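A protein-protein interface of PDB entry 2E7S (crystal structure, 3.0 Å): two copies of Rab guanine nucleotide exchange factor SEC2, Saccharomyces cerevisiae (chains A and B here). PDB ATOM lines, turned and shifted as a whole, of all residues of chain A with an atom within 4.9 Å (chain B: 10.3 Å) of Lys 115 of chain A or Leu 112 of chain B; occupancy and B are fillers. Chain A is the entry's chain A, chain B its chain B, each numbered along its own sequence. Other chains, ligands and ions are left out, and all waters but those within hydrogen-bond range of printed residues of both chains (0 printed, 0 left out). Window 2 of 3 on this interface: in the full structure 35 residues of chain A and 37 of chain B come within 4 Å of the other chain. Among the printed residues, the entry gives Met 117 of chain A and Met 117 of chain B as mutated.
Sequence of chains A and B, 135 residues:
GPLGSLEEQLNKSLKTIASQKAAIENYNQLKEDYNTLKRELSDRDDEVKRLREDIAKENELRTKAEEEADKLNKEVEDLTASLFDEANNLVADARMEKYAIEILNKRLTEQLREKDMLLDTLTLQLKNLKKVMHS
The side-chain amino group (NZ) of Lys 115 of chain A sits close to the backbone carbonyl oxygen (O) of Leu 112 of chain B. The side-chain amino group (NZ) of Lys 115 of chain A lies within salt-bridge range of the side-chain carboxylate (OD1) of Asp 116 of chain B, 3.2 Å away. NZ of Lys 115 of chain A sits close to O of Lys 115 of chain B.
Leu 108 of chain A touches Asn 105 of chain B. Leu 108 of chain A touches Leu 108 of chain B (CB to CD1, 3.4 Å). CD1 of Leu 112 of chain A touches OE1 of Gln 111 of chain B, 2.8 Å away. Leu 112 of chain A touches Leu 112 of chain B. Lys 115 of chain A touches Leu 119 of chain B. Leu 118 of chain B touches Leu 119 of chain A. Leu 119 of chain A touches Leu 119 of chain B (CD1 to CD2, 3.2 Å). Leu 119 of chain A touches Leu 122 of chain B (CD1 to CG, 3.1 Å).
Lys 115 of chain A touches just these residues of chain B: Leu 112, Lys 115, Asp 116 and Leu 119. No residue of chain B comes within 4 Å of Asp 116 of chain A. Leu 119 of chain A touches just these residues of chain B: Leu 118, Leu 119 and Leu 122. Of the printed residues of chain A, Gln 111 of chain B touches Leu 112. Of the printed residues of chain A, Leu 122 of chain B touches Leu 119 (3.1 Å). Printed residues of chain B within 4 Å of Leu 112 of chain A: Gln 111 and Leu 112. Arg 113 of chain B touches none of the printed residues of chain A. Glu 114 of chain B touches none of the printed residues of chain A. The nearest residue of chain B that does not touch Lys 115 of chain A is Gln 111 of chain B (5.3 Å). The nearest residue of chain A that does not touch Leu 112 of chain B is Leu 108 of chain A (4.6 Å). The nearest printed residue of chain B that does not touch Leu 112 of chain A is Leu 108 of chain B (4.01 Å).
Printed residues of chain B that touch a printed residue of chain A: Asn 105, Leu 108, Gln 111, Leu 112, Lys 115, Asp 116, Leu 118, Leu 119 and Leu 122. Hydrophobic or aromatic side chains of chain B within 4 Å of the printed part of chain A: Leu 108, Leu 112, Leu 119 and Leu 122. Printed residues of chain A that touch a printed residue of chain B: Leu 108, Leu 112, Lys 115 and Leu 119. Among the printed residues, 11 pairs touch across the chains.
O of Leu 112 of chain A sits close to OD2 of Asp 116 of chain A, at 2.5 Å. The side-chain carboxylate (OD2) of Asp 116 of chain B lies close to the backbone carbonyl oxygen (O) of Leu 112 of chain B, 2.6 Å away. The backbone carbonyl oxygen (O) of Asn 105 of chain B sits at hydrogen-bond distance from the side-chain hydroxyl (OG1) of Thr 109 of chain B, at 3.3 Å. O of Leu 119 of chain B sits at hydrogen-bond distance from OG1 of Thr 123 of chain B (2.8 Å).
Leu 108 of chain A touches its own counterpart, Leu 108 of chain B. Leu 112 of chain B touches its own counterpart, Leu 112 of chain A. Lys 115 of chain A touches Asp 116 of chain B, but with the chains exchanged Asp 116 of chain A does not touch Lys 115 of chain B (5.4 Å). Leu 119 of chain B touches its own counterpart, Leu 119 of chain A.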
ATOM      1  N   LEU A 108      -6.130  16.793  26.175  1.00  0.00           N
ATOM      2  CA  LEU A 108      -6.342  17.092  24.755  1.00  0.00           C
ATOM      3  C   LEU A 108      -5.069  17.094  23.896  1.00  0.00           C
ATOM      4  O   LEU A 108      -5.114  16.738  22.719  1.00  0.00           O
ATOM      5  CB  LEU A 108      -7.073  18.433  24.598  1.00  0.00           C
ATOM      6  CG  LEU A 108      -8.475  18.515  25.204  1.00  0.00           C
ATOM      7  CD1 LEU A 108      -9.007  19.908  25.024  1.00  0.00           C
ATOM      8  CD2 LEU A 108      -9.402  17.515  24.555  1.00  0.00           C
ATOM      9  N   GLN A 111      -3.927  13.289  24.027  1.00  0.00           N
ATOM     10  CA  GLN A 111      -4.889  12.382  23.385  1.00  0.00           C
ATOM     11  C   GLN A 111      -4.846  12.527  21.872  1.00  0.00           C
ATOM     12  O   GLN A 111      -5.359  11.678  21.141  1.00  0.00           O
ATOM     13  CB  GLN A 111      -6.317  12.648  23.866  1.00  0.00           C
ATOM     14  CG  GLN A 111      -6.687  11.956  25.169  1.00  0.00           C
ATOM     15  CD  GLN A 111      -8.130  12.211  25.567  1.00  0.00           C
ATOM     16  OE1 GLN A 111      -9.052  11.967  24.785  1.00  0.00           O
ATOM     17  NE2 GLN A 111      -8.333  12.702  26.788  1.00  0.00           N
ATOM     18  N   LEU A 112      -4.254  13.621  21.406  1.00  0.00           N
ATOM     19  CA  LEU A 112      -4.111  13.848  19.978  1.00  0.00           C
ATOM     20  C   LEU A 112      -2.806  13.173  19.548  1.00  0.00           C
ATOM     21  O   LEU A 112      -2.578  12.942  18.360  1.00  0.00           O
ATOM     22  CB  LEU A 112      -4.095  15.345  19.674  1.00  0.00           C
ATOM     23  CG  LEU A 112      -5.456  16.022  19.866  1.00  0.00           C
ATOM     24  CD1 LEU A 112      -5.301  17.514  19.686  1.00  0.00           C
ATOM     25  CD2 LEU A 112      -6.470  15.472  18.880  1.00  0.00           C
ATOM     26  N   ARG A 113      -1.957  12.868  20.531  1.00  0.00           N
ATOM     27  CA  ARG A 113      -0.703  12.153  20.301  1.00  0.00           C
ATOM     28  C   ARG A 113      -1.036  10.686  20.535  1.00  0.00           C
ATOM     29  O   ARG A 113      -0.392   9.797  19.982  1.00  0.00           O
ATOM     30  CB  ARG A 113       0.379  12.574  21.286  1.00  0.00           C
ATOM     31  CG  ARG A 113       1.214  13.717  20.819  1.00  0.00           C
ATOM     32  CD  ARG A 113       2.431  13.825  21.686  1.00  0.00           C
ATOM     33  NE  ARG A 113       3.299  14.911  21.257  1.00  0.00           N
ATOM     34  CZ  ARG A 113       4.456  15.205  21.838  1.00  0.00           C
ATOM     35  NH1 ARG A 113       4.878  14.484  22.871  1.00  0.00           N
ATOM     36  NH2 ARG A 113       5.186  16.221  21.393  1.00  0.00           N
ATOM     37  N   GLU A 114      -2.044  10.454  21.381  1.00  0.00           N
ATOM     38  CA  GLU A 114      -2.543   9.112  21.696  1.00  0.00           C
ATOM     39  C   GLU A 114      -3.351   8.694  20.473  1.00  0.00           C
ATOM     40  O   GLU A 114      -3.706   7.530  20.307  1.00  0.00           O
ATOM     41  CB  GLU A 114      -3.473   9.149  22.919  1.00  0.00           C
ATOM     42  CG  GLU A 114      -4.102   7.806  23.279  1.00  0.00           C
ATOM     43  CD  GLU A 114      -5.343   7.942  24.146  1.00  0.00           C
ATOM     44  OE1 GLU A 114      -6.364   8.456  23.644  1.00  0.00           O
ATOM     45  OE2 GLU A 114      -5.300   7.532  25.326  1.00  0.00           O
ATOM     46  N   LYS A 115      -3.643   9.681  19.630  1.00  0.00           N
ATOM     47  CA  LYS A 115      -4.400   9.488  18.403  1.00  0.00           C
ATOM     48  C   LYS A 115      -3.414   9.333  17.245  1.00  0.00           C
ATOM     49  O   LYS A 115      -3.813   9.191  16.085  1.00  0.00           O
ATOM     50  CB  LYS A 115      -5.291  10.698  18.172  1.00  0.00           C
ATOM     51  CG  LYS A 115      -6.400  10.478  17.203  1.00  0.00           C
ATOM     52  CD  LYS A 115      -7.218  11.730  17.148  1.00  0.00           C
ATOM     53  CE  LYS A 115      -8.478  11.522  16.375  1.00  0.00           C
ATOM     54  NZ  LYS A 115      -9.271  12.773  16.389  1.00  0.00           N
ATOM     55  N   ASP A 116      -2.122   9.376  17.582  1.00  0.00           N
ATOM     56  CA  ASP A 116      -1.030   9.215  16.615  1.00  0.00           C
ATOM     57  C   ASP A 116      -0.308   7.881  16.846  1.00  0.00           C
ATOM     58  O   ASP A 116       0.386   7.384  15.951  1.00  0.00           O
ATOM     59  CB  ASP A 116      -0.015  10.359  16.730  1.00  0.00           C
ATOM     60  CG  ASP A 116      -0.617  11.708  16.407  1.00  0.00           C
ATOM     61  OD1 ASP A 116      -1.272  11.825  15.346  1.00  0.00           O
ATOM     62  OD2 ASP A 116      -0.427  12.649  17.210  1.00  0.00           O
ATOM     63  N   MET A 117      -0.464   7.317  18.049  1.00  0.00           N
ATOM     64  CA  MET A 117       0.144   6.026  18.404  1.00  0.00           C
ATOM     65  C   MET A 117      -0.784   4.879  17.970  1.00  0.00           C
ATOM     66  O   MET A 117      -0.317   3.794  17.599  1.00  0.00           O
ATOM     67  CB  MET A 117       0.389   5.920  19.922  1.00  0.00           C
ATOM     68  CG  MET A 117       1.110   4.613  20.336  1.00  0.00           C
ATOM     69  SD  MET A 117       0.992   4.011  22.217  1.00  0.00           S
ATOM     70  CE  MET A 117       2.490   5.003  22.979  1.00  0.00           C
ATOM     71  N   LEU A 118      -2.095   5.135  18.025  1.00  0.00           N
ATOM     72  CA  LEU A 118      -3.114   4.157  17.639  1.00  0.00           C
ATOM     73  C   LEU A 118      -3.512   4.386  16.175  1.00  0.00           C
ATOM     74  O   LEU A 118      -4.376   3.691  15.636  1.00  0.00           O
ATOM     75  CB  LEU A 118      -4.348   4.289  18.544  1.00  0.00           C
ATOM     76  CG  LEU A 118      -5.356   3.136  18.561  1.00  0.00           C
ATOM     77  CD1 LEU A 118      -4.705   1.892  19.147  1.00  0.00           C
ATOM     78  CD2 LEU A 118      -6.565   3.526  19.385  1.00  0.00           C
ATOM     79  N   LEU A 119      -2.869   5.366  15.540  1.00  0.00           N
ATOM     80  CA  LEU A 119      -3.126   5.702  14.141  1.00  0.00           C
ATOM     81  C   LEU A 119      -1.838   5.698  13.309  1.00  0.00           C
ATOM     82  O   LEU A 119      -1.693   4.800  12.449  1.00  0.00           O
ATOM     83  CB  LEU A 119      -3.774   7.081  14.039  1.00  0.00           C
ATOM     84  CG  LEU A 119      -4.179   7.465  12.624  1.00  0.00           C
ATOM     85  CD1 LEU A 119      -5.257   6.517  12.161  1.00  0.00           C
ATOM     86  CD2 LEU A 119      -4.668   8.885  12.588  1.00  0.00           C
ATOM     87  N   LEU B 104      -7.943  28.019  23.124  1.00  0.00           N
ATOM     88  CA  LEU B 104      -6.971  26.961  22.892  1.00  0.00           C
ATOM     89  C   LEU B 104      -7.615  25.647  23.268  1.00  0.00           C
ATOM     90  O   LEU B 104      -7.564  24.691  22.509  1.00  0.00           O
ATOM     91  CB  LEU B 104      -5.736  27.166  23.758  1.00  0.00           C
ATOM     92  CG  LEU B 104      -4.712  26.028  23.782  1.00  0.00           C
ATOM     93  CD1 LEU B 104      -4.061  25.915  22.421  1.00  0.00           C
ATOM     94  CD2 LEU B 104      -3.653  26.302  24.838  1.00  0.00           C
ATOM     95  N   ASN B 105      -8.217  25.607  24.450  1.00  0.00           N
ATOM     96  CA  ASN B 105      -8.888  24.408  24.932  1.00  0.00           C
ATOM     97  C   ASN B 105     -10.039  24.063  24.016  1.00  0.00           C
ATOM     98  O   ASN B 105     -10.494  22.921  23.981  1.00  0.00           O
ATOM     99  CB  ASN B 105      -9.428  24.612  26.340  1.00  0.00           C
ATOM    100  CG  ASN B 105     -10.337  23.482  26.778  1.00  0.00           C
ATOM    101  OD1 ASN B 105     -11.434  23.316  26.244  1.00  0.00           O
ATOM    102  ND2 ASN B 105      -9.885  22.694  27.753  1.00  0.00           N
ATOM    103  N   LYS B 106     -10.518  25.058  23.282  1.00  0.00           N
ATOM    104  CA  LYS B 106     -11.612  24.839  22.353  1.00  0.00           C
ATOM    105  C   LYS B 106     -11.118  24.776  20.899  1.00  0.00           C
ATOM    106  O   LYS B 106     -11.921  24.737  19.965  1.00  0.00           O
ATOM    107  CB  LYS B 106     -12.663  25.943  22.518  1.00  0.00           C
ATOM    108  CG  LYS B 106     -13.417  25.890  23.843  1.00  0.00           C
ATOM    109  CD  LYS B 106     -14.527  26.934  23.892  1.00  0.00           C
ATOM    110  CE  LYS B 106     -15.346  26.818  25.167  1.00  0.00           C
ATOM    111  NZ  LYS B 106     -16.482  27.787  25.205  1.00  0.00           N
ATOM    112  N   ARG B 107      -9.798  24.754  20.713  1.00  0.00           N
ATOM    113  CA  ARG B 107      -9.215  24.696  19.374  1.00  0.00           C
ATOM    114  C   ARG B 107      -8.799  23.283  19.041  1.00  0.00           C
ATOM    115  O   ARG B 107      -8.711  22.905  17.872  1.00  0.00           O
ATOM    116  CB  ARG B 107      -8.005  25.622  19.272  1.00  0.00           C
ATOM    117  CG  ARG B 107      -7.310  25.575  17.928  1.00  0.00           C
ATOM    118  CD  ARG B 107      -6.089  24.672  17.974  1.00  0.00           C
ATOM    119  NE  ARG B 107      -5.473  24.554  16.660  1.00  0.00           N
ATOM    120  CZ  ARG B 107      -4.237  24.118  16.452  1.00  0.00           C
ATOM    121  NH1 ARG B 107      -3.474  23.761  17.483  1.00  0.00           N
ATOM    122  NH2 ARG B 107      -3.770  24.039  15.212  1.00  0.00           N
ATOM    123  N   LEU B 108      -8.536  22.503  20.078  1.00  0.00           N
ATOM    124  CA  LEU B 108      -8.152  21.120  19.894  1.00  0.00           C
ATOM    125  C   LEU B 108      -9.441  20.324  19.697  1.00  0.00           C
ATOM    126  O   LEU B 108      -9.427  19.206  19.178  1.00  0.00           O
ATOM    127  CB  LEU B 108      -7.386  20.624  21.123  1.00  0.00           C
ATOM    128  CG  LEU B 108      -6.192  21.477  21.571  1.00  0.00           C
ATOM    129  CD1 LEU B 108      -5.554  20.833  22.794  1.00  0.00           C
ATOM    130  CD2 LEU B 108      -5.179  21.628  20.433  1.00  0.00           C
ATOM    131  N   THR B 109     -10.554  20.922  20.112  1.00  0.00           N
ATOM    132  CA  THR B 109     -11.866  20.301  19.987  1.00  0.00           C
ATOM    133  C   THR B 109     -12.362  20.453  18.555  1.00  0.00           C
ATOM    134  O   THR B 109     -12.730  19.474  17.905  1.00  0.00           O
ATOM    135  CB  THR B 109     -12.875  20.963  20.930  1.00  0.00           C
ATOM    136  OG1 THR B 109     -12.435  20.793  22.281  1.00  0.00           O
ATOM    137  CG2 THR B 109     -14.255  20.342  20.762  1.00  0.00           C
ATOM    138  N   GLU B 110     -12.374  21.693  18.075  1.00  0.00           N
ATOM    139  CA  GLU B 110     -12.789  22.008  16.709  1.00  0.00           C
ATOM    140  C   GLU B 110     -11.776  21.368  15.769  1.00  0.00           C
ATOM    141  O   GLU B 110     -11.942  21.380  14.549  1.00  0.00           O
ATOM    142  CB  GLU B 110     -12.781  23.522  16.499  1.00  0.00           C
ATOM    143  CG  GLU B 110     -11.432  24.159  16.830  1.00  0.00           C
ATOM    144  CD  GLU B 110     -11.395  25.659  16.598  1.00  0.00           C
ATOM    145  OE1 GLU B 110     -12.277  26.371  17.129  1.00  0.00           O
ATOM    146  OE2 GLU B 110     -10.474  26.123  15.886  1.00  0.00           O
ATOM    147  N   GLN B 111     -10.718  20.826  16.366  1.00  0.00           N
ATOM    148  CA  GLN B 111      -9.646  20.166  15.644  1.00  0.00           C
ATOM    149  C   GLN B 111      -9.760  18.647  15.772  1.00  0.00           C
ATOM    150  O   GLN B 111      -9.094  17.911  15.045  1.00  0.00           O
ATOM    151  CB  GLN B 111      -8.306  20.626  16.189  1.00  0.00           C
ATOM    152  CG  GLN B 111      -7.137  19.983  15.524  1.00  0.00           C
ATOM    153  CD  GLN B 111      -6.139  19.493  16.529  1.00  0.00           C
ATOM    154  OE1 GLN B 111      -6.413  18.561  17.284  1.00  0.00           O
ATOM    155  NE2 GLN B 111      -4.972  20.123  16.560  1.00  0.00           N
ATOM    156  N   LEU B 112     -10.588  18.180  16.708  1.00  0.00           N
ATOM    157  CA  LEU B 112     -10.805  16.743  16.892  1.00  0.00           C
ATOM    158  C   LEU B 112     -11.808  16.222  15.853  1.00  0.00           C
ATOM    159  O   LEU B 112     -11.781  15.044  15.502  1.00  0.00           O
ATOM    160  CB  LEU B 112     -11.317  16.429  18.305  1.00  0.00           C
ATOM    161  CG  LEU B 112     -10.288  15.978  19.343  1.00  0.00           C
ATOM    162  CD1 LEU B 112     -10.994  15.671  20.638  1.00  0.00           C
ATOM    163  CD2 LEU B 112      -9.562  14.755  18.864  1.00  0.00           C
ATOM    164  N   ARG B 113     -12.690  17.094  15.363  1.00  0.00           N
ATOM    165  CA  ARG B 113     -13.671  16.699  14.348  1.00  0.00           C
ATOM    166  C   ARG B 113     -13.006  16.463  12.989  1.00  0.00           C
ATOM    167  O   ARG B 113     -13.610  15.881  12.085  1.00  0.00           O
ATOM    168  CB  ARG B 113     -14.756  17.770  14.193  1.00  0.00           C
ATOM    169  CG  ARG B 113     -15.849  17.709  15.235  1.00  0.00           C
ATOM    170  CD  ARG B 113     -17.020  18.563  14.804  1.00  0.00           C
ATOM    171  NE  ARG B 113     -18.181  18.362  15.662  1.00  0.00           N
ATOM    172  CZ  ARG B 113     -19.372  18.901  15.433  1.00  0.00           C
ATOM    173  NH1 ARG B 113     -19.552  19.675  14.366  1.00  0.00           N
ATOM    174  NH2 ARG B 113     -20.381  18.665  16.267  1.00  0.00           N
ATOM    175  N   GLU B 114     -11.764  16.922  12.853  1.00  0.00           N
ATOM    176  CA  GLU B 114     -11.005  16.755  11.615  1.00  0.00           C
ATOM    177  C   GLU B 114      -9.984  15.624  11.738  1.00  0.00           C
ATOM    178  O   GLU B 114      -9.088  15.476  10.896  1.00  0.00           O
ATOM    179  CB  GLU B 114     -10.283  18.053  11.250  1.00  0.00           C
ATOM    180  CG  GLU B 114     -11.207  19.199  10.883  1.00  0.00           C
ATOM    181  CD  GLU B 114     -10.440  20.428  10.431  1.00  0.00           C
ATOM    182  OE1 GLU B 114      -9.709  20.341   9.419  1.00  0.00           O
ATOM    183  OE2 GLU B 114     -10.566  21.480  11.093  1.00  0.00           O
ATOM    184  N   LYS B 115     -10.123  14.839  12.801  1.00  0.00           N
ATOM    185  CA  LYS B 115      -9.244  13.704  13.045  1.00  0.00           C
ATOM    186  C   LYS B 115      -9.972  12.526  13.702  1.00  0.00           C
ATOM    187  O   LYS B 115      -9.436  11.416  13.739  1.00  0.00           O
ATOM    188  CB  LYS B 115      -8.040  14.127  13.886  1.00  0.00           C
ATOM    189  CG  LYS B 115      -7.117  15.060  13.143  1.00  0.00           C
ATOM    190  CD  LYS B 115      -5.858  15.323  13.916  1.00  0.00           C
ATOM    191  CE  LYS B 115      -4.940  16.223  13.120  1.00  0.00           C
ATOM    192  NZ  LYS B 115      -3.664  16.476  13.835  1.00  0.00           N
ATOM    193  N   ASP B 116     -11.183  12.762  14.217  1.00  0.00           N
ATOM    194  CA  ASP B 116     -11.989  11.696  14.835  1.00  0.00           C
ATOM    195  C   ASP B 116     -12.680  10.901  13.719  1.00  0.00           C
ATOM    196  O   ASP B 116     -12.903   9.689  13.833  1.00  0.00           O
ATOM    197  CB  ASP B 116     -13.053  12.278  15.782  1.00  0.00           C
ATOM    198  CG  ASP B 116     -12.502  12.600  17.171  1.00  0.00           C
ATOM    199  OD1 ASP B 116     -11.942  11.686  17.821  1.00  0.00           O
ATOM    200  OD2 ASP B 116     -12.639  13.764  17.619  1.00  0.00           O
ATOM    201  N   MET B 117     -13.019  11.607  12.640  1.00  0.00           N
ATOM    202  CA  MET B 117     -13.658  11.003  11.476  1.00  0.00           C
ATOM    203  C   MET B 117     -12.583  10.222  10.712  1.00  0.00           C
ATOM    204  O   MET B 117     -12.890   9.249  10.023  1.00  0.00           O
ATOM    205  CB  MET B 117     -14.241  12.093  10.560  1.00  0.00           C
ATOM    206  CG  MET B 117     -15.250  13.054  11.216  1.00  0.00           C
ATOM    207  SD  MET B 117     -17.126  12.465  11.350  1.00  0.00           S
ATOM    208  CE  MET B 117     -17.769  13.074   9.628  1.00  0.00           C
ATOM    209  N   LEU B 118     -11.327  10.658  10.854  1.00  0.00           N
ATOM    210  CA  LEU B 118     -10.173  10.040  10.187  1.00  0.00           C
ATOM    211  C   LEU B 118      -9.592   8.795  10.897  1.00  0.00           C
ATOM    212  O   LEU B 118      -8.423   8.436  10.703  1.00  0.00           O
ATOM    213  CB  LEU B 118      -9.063  11.093   9.968  1.00  0.00           C
ATOM    214  CG  LEU B 118      -9.421  12.394   9.221  1.00  0.00           C
ATOM    215  CD1 LEU B 118      -8.185  13.283   9.093  1.00  0.00           C
ATOM    216  CD2 LEU B 118      -9.979  12.075   7.846  1.00  0.00           C
ATOM    217  N   LEU B 119     -10.409   8.150  11.729  1.00  0.00           N
ATOM    218  CA  LEU B 119     -10.004   6.927  12.412  1.00  0.00           C
ATOM    219  C   LEU B 119     -11.003   5.841  12.026  1.00  0.00           C
ATOM    220  O   LEU B 119     -10.694   4.651  12.107  1.00  0.00           O
ATOM    221  CB  LEU B 119      -9.975   7.101  13.929  1.00  0.00           C
ATOM    222  CG  LEU B 119      -8.909   8.051  14.475  1.00  0.00           C
ATOM    223  CD1 LEU B 119      -8.628   7.694  15.923  1.00  0.00           C
ATOM    224  CD2 LEU B 119      -7.635   7.948  13.658  1.00  0.00           C
ATOM    225  N   ASP B 120     -12.197   6.260  11.602  1.00  0.00           N
ATOM    226  CA  ASP B 120     -13.246   5.335  11.157  1.00  0.00           C
ATOM    227  C   ASP B 120     -12.917   4.928   9.713  1.00  0.00           C
ATOM    228  O   ASP B 120     -13.473   3.964   9.180  1.00  0.00           O
ATOM    229  CB  ASP B 120     -14.630   6.013  11.175  1.00  0.00           C
ATOM    230  CG  ASP B 120     -15.002   6.579  12.537  1.00  0.00           C
ATOM    231  OD1 ASP B 120     -14.998   5.819  13.525  1.00  0.00           O
ATOM    232  OD2 ASP B 120     -15.313   7.786  12.618  1.00  0.00           O
ATOM    233  N   THR B 121     -12.008   5.688   9.098  1.00  0.00           N
ATOM    234  CA  THR B 121     -11.575   5.466   7.717  1.00  0.00           C
ATOM    235  C   THR B 121     -10.112   4.996   7.587  1.00  0.00           C
ATOM    236  O   THR B 121      -9.779   4.302   6.629  1.00  0.00           O
ATOM    237  CB  THR B 121     -11.774   6.754   6.853  1.00  0.00           C
ATOM    238  OG1 THR B 121     -13.155   7.138   6.871  1.00  0.00           O
ATOM    239  CG2 THR B 121     -11.351   6.509   5.408  1.00  0.00           C
ATOM    240  N   LEU B 122      -9.237   5.369   8.525  1.00  0.00           N
ATOM    241  CA  LEU B 122      -7.839   4.925   8.459  1.00  0.00           C
ATOM    242  C   LEU B 122      -7.864   3.459   8.869  1.00  0.00           C
ATOM    243  O   LEU B 122      -6.836   2.779   8.920  1.00  0.00           O
ATOM    244  CB  LEU B 122      -6.948   5.730   9.415  1.00  0.00           C
ATOM    245  CG  LEU B 122      -5.443   5.806   9.102  1.00  0.00           C
ATOM    246  CD1 LEU B 122      -4.755   4.481   9.383  1.00  0.00           C
ATOM    247  CD2 LEU B 122      -5.254   6.226   7.653  1.00  0.00           C
ATOM    248  N   THR B 123      -9.074   2.997   9.170  1.00  0.00           N
ATOM    249  CA  THR B 123      -9.337   1.617   9.543  1.00  0.00           C
ATOM    250  C   THR B 123     -10.158   0.998   8.392  1.00  0.00           C
ATOM    251  O   THR B 123     -10.429  -0.208   8.376  1.00  0.00           O
ATOM    252  CB  THR B 123     -10.125   1.543  10.867  1.00  0.00           C
ATOM    253  OG1 THR B 123      -9.388   2.221  11.890  1.00  0.00           O
ATOM    254  CG2 THR B 123     -10.332   0.096  11.292  1.00  0.00           C
